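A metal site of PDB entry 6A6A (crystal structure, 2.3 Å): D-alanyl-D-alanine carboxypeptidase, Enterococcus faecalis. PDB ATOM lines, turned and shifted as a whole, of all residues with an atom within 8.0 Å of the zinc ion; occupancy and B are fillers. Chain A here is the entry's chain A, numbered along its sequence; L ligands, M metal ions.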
ATOM      1  N   SER A  92      -4.099  -0.109  10.683  1.00  0.00           N
ATOM      2  CA  SER A  92      -3.971  -0.345   9.246  1.00  0.00           C
ATOM      3  C   SER A  92      -4.564  -1.694   8.860  1.00  0.00           C
ATOM      4  O   SER A  92      -4.260  -2.710   9.487  1.00  0.00           O
ATOM      5  CB  SER A  92      -2.507  -0.241   8.843  1.00  0.00           C
ATOM      6  OG  SER A  92      -2.377  -0.346   7.438  1.00  0.00           O
ATOM      7  N   GLY A  93      -5.376  -1.682   7.809  1.00  0.00           N
ATOM      8  CA  GLY A  93      -6.049  -2.848   7.259  1.00  0.00           C
ATOM      9  C   GLY A  93      -5.551  -3.150   5.856  1.00  0.00           C
ATOM     10  O   GLY A  93      -4.357  -3.309   5.631  1.00  0.00           O
ATOM     11  N   ARG A  95      -4.178  -2.291   2.330  1.00  0.00           N
ATOM     12  CA  ARG A  95      -3.438  -1.187   1.694  1.00  0.00           C
ATOM     13  C   ARG A  95      -3.263  -1.517   0.219  1.00  0.00           C
ATOM     14  O   ARG A  95      -2.963  -2.663  -0.114  1.00  0.00           O
ATOM     15  CB  ARG A  95      -2.008  -1.032   2.232  1.00  0.00           C
ATOM     16  CG  ARG A  95      -1.871  -0.743   3.721  1.00  0.00           C
ATOM     17  CD  ARG A  95      -0.432  -1.025   4.107  1.00  0.00           C
ATOM     18  NE  ARG A  95      -0.186  -0.712   5.504  1.00  0.00           N
ATOM     19  CZ  ARG A  95       0.602  -1.397   6.305  1.00  0.00           C
ATOM     20  NH1 ARG A  95       1.627  -2.091   5.818  1.00  0.00           N
ATOM     21  NH2 ARG A  95       0.354  -1.380   7.611  1.00  0.00           N
ATOM     22  N   GLN A 100       1.362   1.089  -0.027  1.00  0.00           N
ATOM     23  CA  GLN A 100       2.492   0.333   0.484  1.00  0.00           C
ATOM     24  C   GLN A 100       3.817   0.987   0.083  1.00  0.00           C
ATOM     25  O   GLN A 100       4.792   0.906   0.835  1.00  0.00           O
ATOM     26  CB  GLN A 100       2.456  -1.111  -0.009  1.00  0.00           C
ATOM     27  CG  GLN A 100       3.491  -1.982   0.687  1.00  0.00           C
ATOM     28  CD  GLN A 100       3.288  -2.070   2.184  1.00  0.00           C
ATOM     29  OE1 GLN A 100       2.188  -1.922   2.697  1.00  0.00           O
ATOM     30  NE2 GLN A 100       4.363  -2.357   2.897  1.00  0.00           N
ATOM     31  N   ILE A 103       4.232   4.298   2.570  1.00  0.00           N
ATOM     32  CA  ILE A 103       4.754   3.829   3.869  1.00  0.00           C
ATOM     33  C   ILE A 103       6.237   3.464   3.724  1.00  0.00           C
ATOM     34  O   ILE A 103       7.064   3.933   4.477  1.00  0.00           O
ATOM     35  CB  ILE A 103       3.924   2.645   4.416  1.00  0.00           C
ATOM     36  CG1 ILE A 103       2.457   3.021   4.598  1.00  0.00           C
ATOM     37  CG2 ILE A 103       4.501   2.078   5.699  1.00  0.00           C
ATOM     38  CD1 ILE A 103       1.507   1.823   4.728  1.00  0.00           C
ATOM     39  N   TRP A 128      11.327  -3.351   8.094  1.00  0.00           N
ATOM     40  CA  TRP A 128      10.134  -2.821   8.811  1.00  0.00           C
ATOM     41  C   TRP A 128       8.883  -2.807   7.930  1.00  0.00           C
ATOM     42  O   TRP A 128       7.760  -2.845   8.426  1.00  0.00           O
ATOM     43  CB  TRP A 128      10.434  -1.427   9.399  1.00  0.00           C
ATOM     44  CG  TRP A 128      11.424  -1.523  10.510  1.00  0.00           C
ATOM     45  CD1 TRP A 128      12.769  -1.295  10.457  1.00  0.00           C
ATOM     46  CD2 TRP A 128      11.161  -2.023  11.833  1.00  0.00           C
ATOM     47  NE1 TRP A 128      13.343  -1.563  11.667  1.00  0.00           N
ATOM     48  CE2 TRP A 128      12.380  -2.024  12.525  1.00  0.00           C
ATOM     49  CE3 TRP A 128       9.994  -2.440  12.489  1.00  0.00           C
ATOM     50  CZ2 TRP A 128      12.474  -2.423  13.854  1.00  0.00           C
ATOM     51  CZ3 TRP A 128      10.080  -2.840  13.803  1.00  0.00           C
ATOM     52  CH2 TRP A 128      11.311  -2.822  14.473  1.00  0.00           C
ATOM     53  N   VAL A 129       9.088  -2.739   6.627  1.00  0.00           N
ATOM     54  CA  VAL A 129       8.037  -2.443   5.659  1.00  0.00           C
ATOM     55  C   VAL A 129       8.316  -3.298   4.425  1.00  0.00           C
ATOM     56  O   VAL A 129       9.450  -3.281   3.924  1.00  0.00           O
ATOM     57  CB  VAL A 129       7.989  -0.943   5.349  1.00  0.00           C
ATOM     58  CG1 VAL A 129       7.079  -0.624   4.172  1.00  0.00           C
ATOM     59  CG2 VAL A 129       7.593  -0.107   6.558  1.00  0.00           C
ATOM     60  N   ALA A 130       7.307  -4.059   3.990  1.00  0.00           N
ATOM     61  CA  ALA A 130       7.415  -4.966   2.871  1.00  0.00           C
ATOM     62  C   ALA A 130       7.393  -4.136   1.588  1.00  0.00           C
ATOM     63  O   ALA A 130       6.630  -3.157   1.467  1.00  0.00           O
ATOM     64  CB  ALA A 130       6.276  -5.941   2.916  1.00  0.00           C
ATOM     65  N   SER A 135       3.408  -7.087   0.748  1.00  0.00           N
ATOM     66  CA  SER A 135       2.762  -6.896   2.045  1.00  0.00           C
ATOM     67  C   SER A 135       1.487  -7.725   2.101  1.00  0.00           C
ATOM     68  O   SER A 135       0.689  -7.659   1.189  1.00  0.00           O
ATOM     69  CB  SER A 135       2.444  -5.467   2.369  1.00  0.00           C
ATOM     70  OG  SER A 135       1.709  -5.391   3.587  1.00  0.00           O
ATOM     71  N   GLU A 136       1.301  -8.445   3.212  1.00  0.00           N
ATOM     72  CA  GLU A 136       0.077  -9.147   3.513  1.00  0.00           C
ATOM     73  C   GLU A 136      -1.110  -8.175   3.514  1.00  0.00           C
ATOM     74  O   GLU A 136      -2.247  -8.606   3.261  1.00  0.00           O
ATOM     75  CB  GLU A 136       0.092  -9.769   4.908  1.00  0.00           C
ATOM     76  CG  GLU A 136       1.086 -10.881   5.077  1.00  0.00           C
ATOM     77  CD  GLU A 136       0.974 -11.530   6.440  1.00  0.00           C
ATOM     78  OE1 GLU A 136       0.833 -10.803   7.440  1.00  0.00           O
ATOM     79  OE2 GLU A 136       1.047 -12.750   6.503  1.00  0.00           O
ATOM     80  N   HIS A 137      -0.842  -6.907   3.859  1.00  0.00           N
ATOM     81  CA  HIS A 137      -1.860  -5.882   3.958  1.00  0.00           C
ATOM     82  C   HIS A 137      -2.547  -5.713   2.601  1.00  0.00           C
ATOM     83  O   HIS A 137      -3.663  -5.185   2.528  1.00  0.00           O
ATOM     84  CB  HIS A 137      -1.264  -4.555   4.417  1.00  0.00           C
ATOM     85  CG  HIS A 137      -0.965  -4.498   5.875  1.00  0.00           C
ATOM     86  ND1 HIS A 137      -1.845  -3.953   6.772  1.00  0.00           N
ATOM     87  CD2 HIS A 137       0.105  -4.893   6.574  1.00  0.00           C
ATOM     88  CE1 HIS A 137      -1.347  -4.046   7.983  1.00  0.00           C
ATOM     89  NE2 HIS A 137      -0.134  -4.612   7.898  1.00  0.00           N
ATOM     90  N   ALA A 142      -4.271  -8.886   6.779  1.00  0.00           N
ATOM     91  CA  ALA A 142      -3.437  -8.357   7.848  1.00  0.00           C
ATOM     92  C   ALA A 142      -4.088  -7.107   8.445  1.00  0.00           C
ATOM     93  O   ALA A 142      -4.559  -6.202   7.724  1.00  0.00           O
ATOM     94  CB  ALA A 142      -2.060  -8.051   7.336  1.00  0.00           C
ATOM     95  N   VAL A 143      -4.108  -7.068   9.772  1.00  0.00           N
ATOM     96  CA  VAL A 143      -4.380  -5.813  10.492  1.00  0.00           C
ATOM     97  C   VAL A 143      -3.182  -5.500  11.401  1.00  0.00           C
ATOM     98  O   VAL A 143      -2.567  -6.411  11.994  1.00  0.00           O
ATOM     99  CB  VAL A 143      -5.703  -5.834  11.280  1.00  0.00           C
ATOM    100  CG1 VAL A 143      -6.900  -5.800  10.353  1.00  0.00           C
ATOM    101  CG2 VAL A 143      -5.788  -7.011  12.230  1.00  0.00           C
ATOM    102  N   ASP A 144      -2.877  -4.211  11.463  1.00  0.00           N
ATOM    103  CA  ASP A 144      -1.952  -3.626  12.402  1.00  0.00           C
ATOM    104  C   ASP A 144      -2.814  -3.049  13.527  1.00  0.00           C
ATOM    105  O   ASP A 144      -3.565  -2.114  13.289  1.00  0.00           O
ATOM    106  CB  ASP A 144      -1.140  -2.508  11.744  1.00  0.00           C
ATOM    107  CG  ASP A 144      -0.122  -3.007  10.750  1.00  0.00           C
ATOM    108  OD1 ASP A 144       0.317  -4.124  10.942  1.00  0.00           O
ATOM    109  OD2 ASP A 144       0.218  -2.270   9.809  1.00  0.00           O
ATOM    110  N   ILE A 145      -2.756  -3.703  14.686  1.00  0.00           N
ATOM    111  CA  ILE A 145      -3.539  -3.345  15.799  1.00  0.00           C
ATOM    112  C   ILE A 145      -2.677  -2.537  16.794  1.00  0.00           C
ATOM    113  O   ILE A 145      -1.551  -2.896  17.119  1.00  0.00           O
ATOM    114  CB  ILE A 145      -4.134  -4.608  16.440  1.00  0.00           C
ATOM    115  CG1 ILE A 145      -4.924  -5.450  15.434  1.00  0.00           C
ATOM    116  CG2 ILE A 145      -5.015  -4.240  17.622  1.00  0.00           C
ATOM    117  CD1 ILE A 145      -5.047  -6.919  15.839  1.00  0.00           C
ATOM    118  N   ARG A 173       2.496 -12.256  13.431  1.00  0.00           N
ATOM    119  CA  ARG A 173       3.121 -12.620  12.195  1.00  0.00           C
ATOM    120  C   ARG A 173       4.637 -12.547  12.298  1.00  0.00           C
ATOM    121  O   ARG A 173       5.338 -13.325  11.650  1.00  0.00           O
ATOM    122  CB  ARG A 173       2.656 -11.674  11.087  1.00  0.00           C
ATOM    123  CG  ARG A 173       3.048 -12.114   9.691  1.00  0.00           C
ATOM    124  CD  ARG A 173       2.752 -13.557   9.285  1.00  0.00           C
ATOM    125  NE  ARG A 173       3.321 -13.850   7.975  1.00  0.00           N
ATOM    126  CZ  ARG A 173       4.529 -14.366   7.721  1.00  0.00           C
ATOM    127  NH1 ARG A 173       5.415 -14.566   8.694  1.00  0.00           N
ATOM    128  NH2 ARG A 173       4.821 -14.717   6.487  1.00  0.00           N
ATOM    129  N   TYR A 174       5.145 -11.560  13.052  1.00  0.00           N
ATOM    130  CA  TYR A 174       6.558 -11.199  12.974  1.00  0.00           C
ATOM    131  C   TYR A 174       7.144 -11.154  14.376  1.00  0.00           C
ATOM    132  O   TYR A 174       7.597 -10.120  14.849  1.00  0.00           O
ATOM    133  CB  TYR A 174       6.726  -9.867  12.256  1.00  0.00           C
ATOM    134  CG  TYR A 174       6.190  -9.847  10.847  1.00  0.00           C
ATOM    135  CD1 TYR A 174       6.653 -10.768   9.901  1.00  0.00           C
ATOM    136  CD2 TYR A 174       5.213  -8.943  10.461  1.00  0.00           C
ATOM    137  CE1 TYR A 174       6.156 -10.780   8.612  1.00  0.00           C
ATOM    138  CE2 TYR A 174       4.706  -8.942   9.170  1.00  0.00           C
ATOM    139  CZ  TYR A 174       5.188  -9.868   8.247  1.00  0.00           C
ATOM    140  OH  TYR A 174       4.688  -9.872   6.979  1.00  0.00           O
ATOM    141  N   VAL A 184      11.600  -9.848   8.766  1.00  0.00           N
ATOM    142  CA  VAL A 184      10.940  -8.648   9.265  1.00  0.00           C
ATOM    143  C   VAL A 184      11.203  -8.561  10.760  1.00  0.00           C
ATOM    144  O   VAL A 184      11.087  -9.566  11.458  1.00  0.00           O
ATOM    145  CB  VAL A 184       9.418  -8.649   8.999  1.00  0.00           C
ATOM    146  CG1 VAL A 184       8.777  -7.331   9.363  1.00  0.00           C
ATOM    147  CG2 VAL A 184       9.067  -9.038   7.568  1.00  0.00           C
ATOM    148  N   GLU A 187       7.386  -6.696  15.063  1.00  0.00           N
ATOM    149  CA  GLU A 187       6.256  -5.855  14.730  1.00  0.00           C
ATOM    150  C   GLU A 187       5.056  -6.326  15.536  1.00  0.00           C
ATOM    151  O   GLU A 187       4.202  -7.072  15.058  1.00  0.00           O
ATOM    152  CB  GLU A 187       6.021  -5.864  13.225  1.00  0.00           C
ATOM    153  CG  GLU A 187       7.219  -5.393  12.433  1.00  0.00           C
ATOM    154  CD  GLU A 187       6.956  -4.506  11.235  1.00  0.00           C
ATOM    155  OE1 GLU A 187       6.011  -3.703  11.280  1.00  0.00           O
ATOM    156  OE2 GLU A 187       7.725  -4.576  10.277  1.00  0.00           O
ATOM    157  N   TRP A 189       2.297  -5.160  16.441  1.00  0.00           N
ATOM    158  CA  TRP A 189       0.974  -4.720  15.948  1.00  0.00           C
ATOM    159  C   TRP A 189       0.440  -5.622  14.815  1.00  0.00           C
ATOM    160  O   TRP A 189      -0.731  -5.684  14.574  1.00  0.00           O
ATOM    161  CB  TRP A 189       1.052  -3.263  15.490  1.00  0.00           C
ATOM    162  CG  TRP A 189       2.263  -3.008  14.644  1.00  0.00           C
ATOM    163  CD1 TRP A 189       2.369  -3.202  13.308  1.00  0.00           C
ATOM    164  CD2 TRP A 189       3.541  -2.504  15.076  1.00  0.00           C
ATOM    165  NE1 TRP A 189       3.628  -2.899  12.877  1.00  0.00           N
ATOM    166  CE2 TRP A 189       4.375  -2.465  13.938  1.00  0.00           C
ATOM    167  CE3 TRP A 189       4.083  -2.112  16.298  1.00  0.00           C
ATOM    168  CZ2 TRP A 189       5.702  -2.031  13.995  1.00  0.00           C
ATOM    169  CZ3 TRP A 189       5.400  -1.699  16.363  1.00  0.00           C
ATOM    170  CH2 TRP A 189       6.194  -1.661  15.221  1.00  0.00           C
ATOM    171  N   HIS A 190       1.318  -6.248  14.059  1.00  0.00           N
ATOM    172  CA  HIS A 190       0.936  -6.837  12.811  1.00  0.00           C
ATOM    173  C   HIS A 190       0.446  -8.264  13.040  1.00  0.00           C
ATOM    174  O   HIS A 190       1.244  -9.146  13.393  1.00  0.00           O
ATOM    175  CB  HIS A 190       2.075  -6.772  11.822  1.00  0.00           C
ATOM    176  CG  HIS A 190       1.710  -7.331  10.495  1.00  0.00           C
ATOM    177  ND1 HIS A 190       1.428  -6.534   9.417  1.00  0.00           N
ATOM    178  CD2 HIS A 190       1.612  -8.621  10.076  1.00  0.00           C
ATOM    179  CE1 HIS A 190       1.172  -7.316   8.381  1.00  0.00           C
ATOM    180  NE2 HIS A 190       1.266  -8.603   8.772  1.00  0.00           N
ATOM    181  N   TYR A 191      -0.863  -8.434  12.815  1.00  0.00           N
ATOM    182  CA  TYR A 191      -1.567  -9.677  13.016  1.00  0.00           C
ATOM    183  C   TYR A 191      -2.164 -10.165  11.667  1.00  0.00           C
ATOM    184  O   TYR A 191      -2.756  -9.417  10.896  1.00  0.00           O
ATOM    185  CB  TYR A 191      -2.560  -9.498  14.172  1.00  0.00           C
ATOM    186  CG  TYR A 191      -1.858  -9.684  15.489  1.00  0.00           C
ATOM    187  CD1 TYR A 191      -1.124  -8.663  16.077  1.00  0.00           C
ATOM    188  CD2 TYR A 191      -1.825 -10.936  16.078  1.00  0.00           C
ATOM    189  CE1 TYR A 191      -0.407  -8.867  17.247  1.00  0.00           C
ATOM    190  CE2 TYR A 191      -1.108 -11.162  17.242  1.00  0.00           C
ATOM    191  CZ  TYR A 191      -0.404 -10.120  17.833  1.00  0.00           C
ATOM    192  OH  TYR A 191       0.266 -10.390  18.982  1.00  0.00           O
ATOM    193  N   ARG A 192      -1.954 -11.438  11.378  1.00  0.00           N
ATOM    194  CA  ARG A 192      -2.317 -12.019  10.138  1.00  0.00           C
ATOM    195  C   ARG A 192      -3.416 -13.053  10.412  1.00  0.00           C
ATOM    196  O   ARG A 192      -3.218 -13.962  11.256  1.00  0.00           O
ATOM    197  CB  ARG A 192      -1.087 -12.677   9.498  1.00  0.00           C
ATOM    198  CG  ARG A 192      -1.402 -13.718   8.433  1.00  0.00           C
ATOM    199  CD  ARG A 192      -2.158 -13.183   7.241  1.00  0.00           C
ATOM    200  NE  ARG A 192      -2.612 -14.295   6.396  1.00  0.00           N
ATOM    201  CZ  ARG A 192      -1.888 -14.897   5.452  1.00  0.00           C
ATOM    202  NH1 ARG A 192      -0.613 -14.576   5.263  1.00  0.00           N
ATOM    203  NH2 ARG A 192      -2.467 -15.794   4.677  1.00  0.00           N
HETATM  204  C1  LIG L   1       3.247  -2.984   8.983  1.00  0.00           C
HETATM  205  O1  LIG L   1       2.409  -3.162   8.043  1.00  0.00           O
HETATM  206  O2  LIG L   1       3.178  -3.699  10.027  1.00  0.00           O
HETATM  207  C2  LIG L   1       4.327  -1.921   8.890  1.00  0.00           C
HETATM  208  N1  LG2 L   2       6.033  -4.748   7.484  1.00  0.00           N
HETATM  209  C1  LG2 L   2       4.910  -5.613   7.123  1.00  0.00           C
HETATM  210  C2  LG2 L   2       5.678  -6.761   6.531  1.00  0.00           C
HETATM  211  C3  LG2 L   2       4.155  -4.960   5.994  1.00  0.00           C
HETATM  212  O1  LG2 L   2       4.512  -3.926   5.389  1.00  0.00           O
HETATM  213  O2  LG2 L   2       3.156  -5.512   5.593  1.00  0.00           O
HETATM  214 ZN    ZN M   1       1.350  -4.583   9.269  1.00  0.00          ZN
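The guanidinium group (NH1) of Arg 95 lies within salt-bridge range of an oxygen (O1) of LG2 L2 (3.4 Å). OE2 of Glu 187 lies within salt-bridge range of N1 of LG2 L2, at 3.3 Å. O2 of LG2 L2 sits at hydrogen-bond distance from OG of Ser 135 (2.5 Å). A nitrogen (N1) of LG2 L2 is in hydrogen-bond range of the backbone carbonyl oxygen (O) of Trp 128, at 2.7 Å. An oxygen (O1) of LG2 L2 lies within hydrogen-bond range of the side-chain amide nitrogen (NE2) of Gln 100 (2.9 Å). N of Ala 130 sits at hydrogen-bond distance from O1 of LG2 L2, 3.1 Å away.
NE2 of His 190 is in hydrogen-bond range of OE1 of Glu 136, at 2.6 Å. The backbone NH of Arg 173 lies within hydrogen-bond range of the backbone carbonyl oxygen of His 190, at 3.4 Å. The backbone NH of Asp 144 is in hydrogen-bond range of the backbone carbonyl oxygen of Ser 92, 2.8 Å away. N of Arg 95 sits at hydrogen-bond distance from O of His 137. The side-chain hydroxyl (OG) of Ser 135 lies within hydrogen-bond range of the backbone NH (N) of His 137 (3.0 Å). The backbone carbonyl oxygen (O) of Gly 93 sits at hydrogen-bond distance from a ring nitrogen (ND1) of His 137 (2.8 Å). The guanidinium group (NH2) of Arg 95 sits at hydrogen-bond distance from the side-chain hydroxyl (OG) of Ser 92 (2.9 Å). NH1 of Arg 95 lies close to OE1 of Gln 100, 3.2 Å away.
Residues that only touch the zinc ion: Arg 95 (3.7 Å). Of the 23 residues printed, 4 come within 4 Å of the zinc ion. The nearest printed residue that does not touch the zinc ion is Trp 189 (4.4 Å).
The zinc ion is bound by a ring nitrogen (ND1) of His 190 (2.0 Å), the side-chain carboxylate (OD1) of Asp 144 (2.0 Å), a ring nitrogen (NE2) of His 137 (2.0 Å), an oxygen (O1) of LIG L1 (2.2 Å) and an oxygen (O2) of LIG L1 (2.2 Å). Slightly farther from the zinc ion lies OD2 of Asp 144 (2.6 Å).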
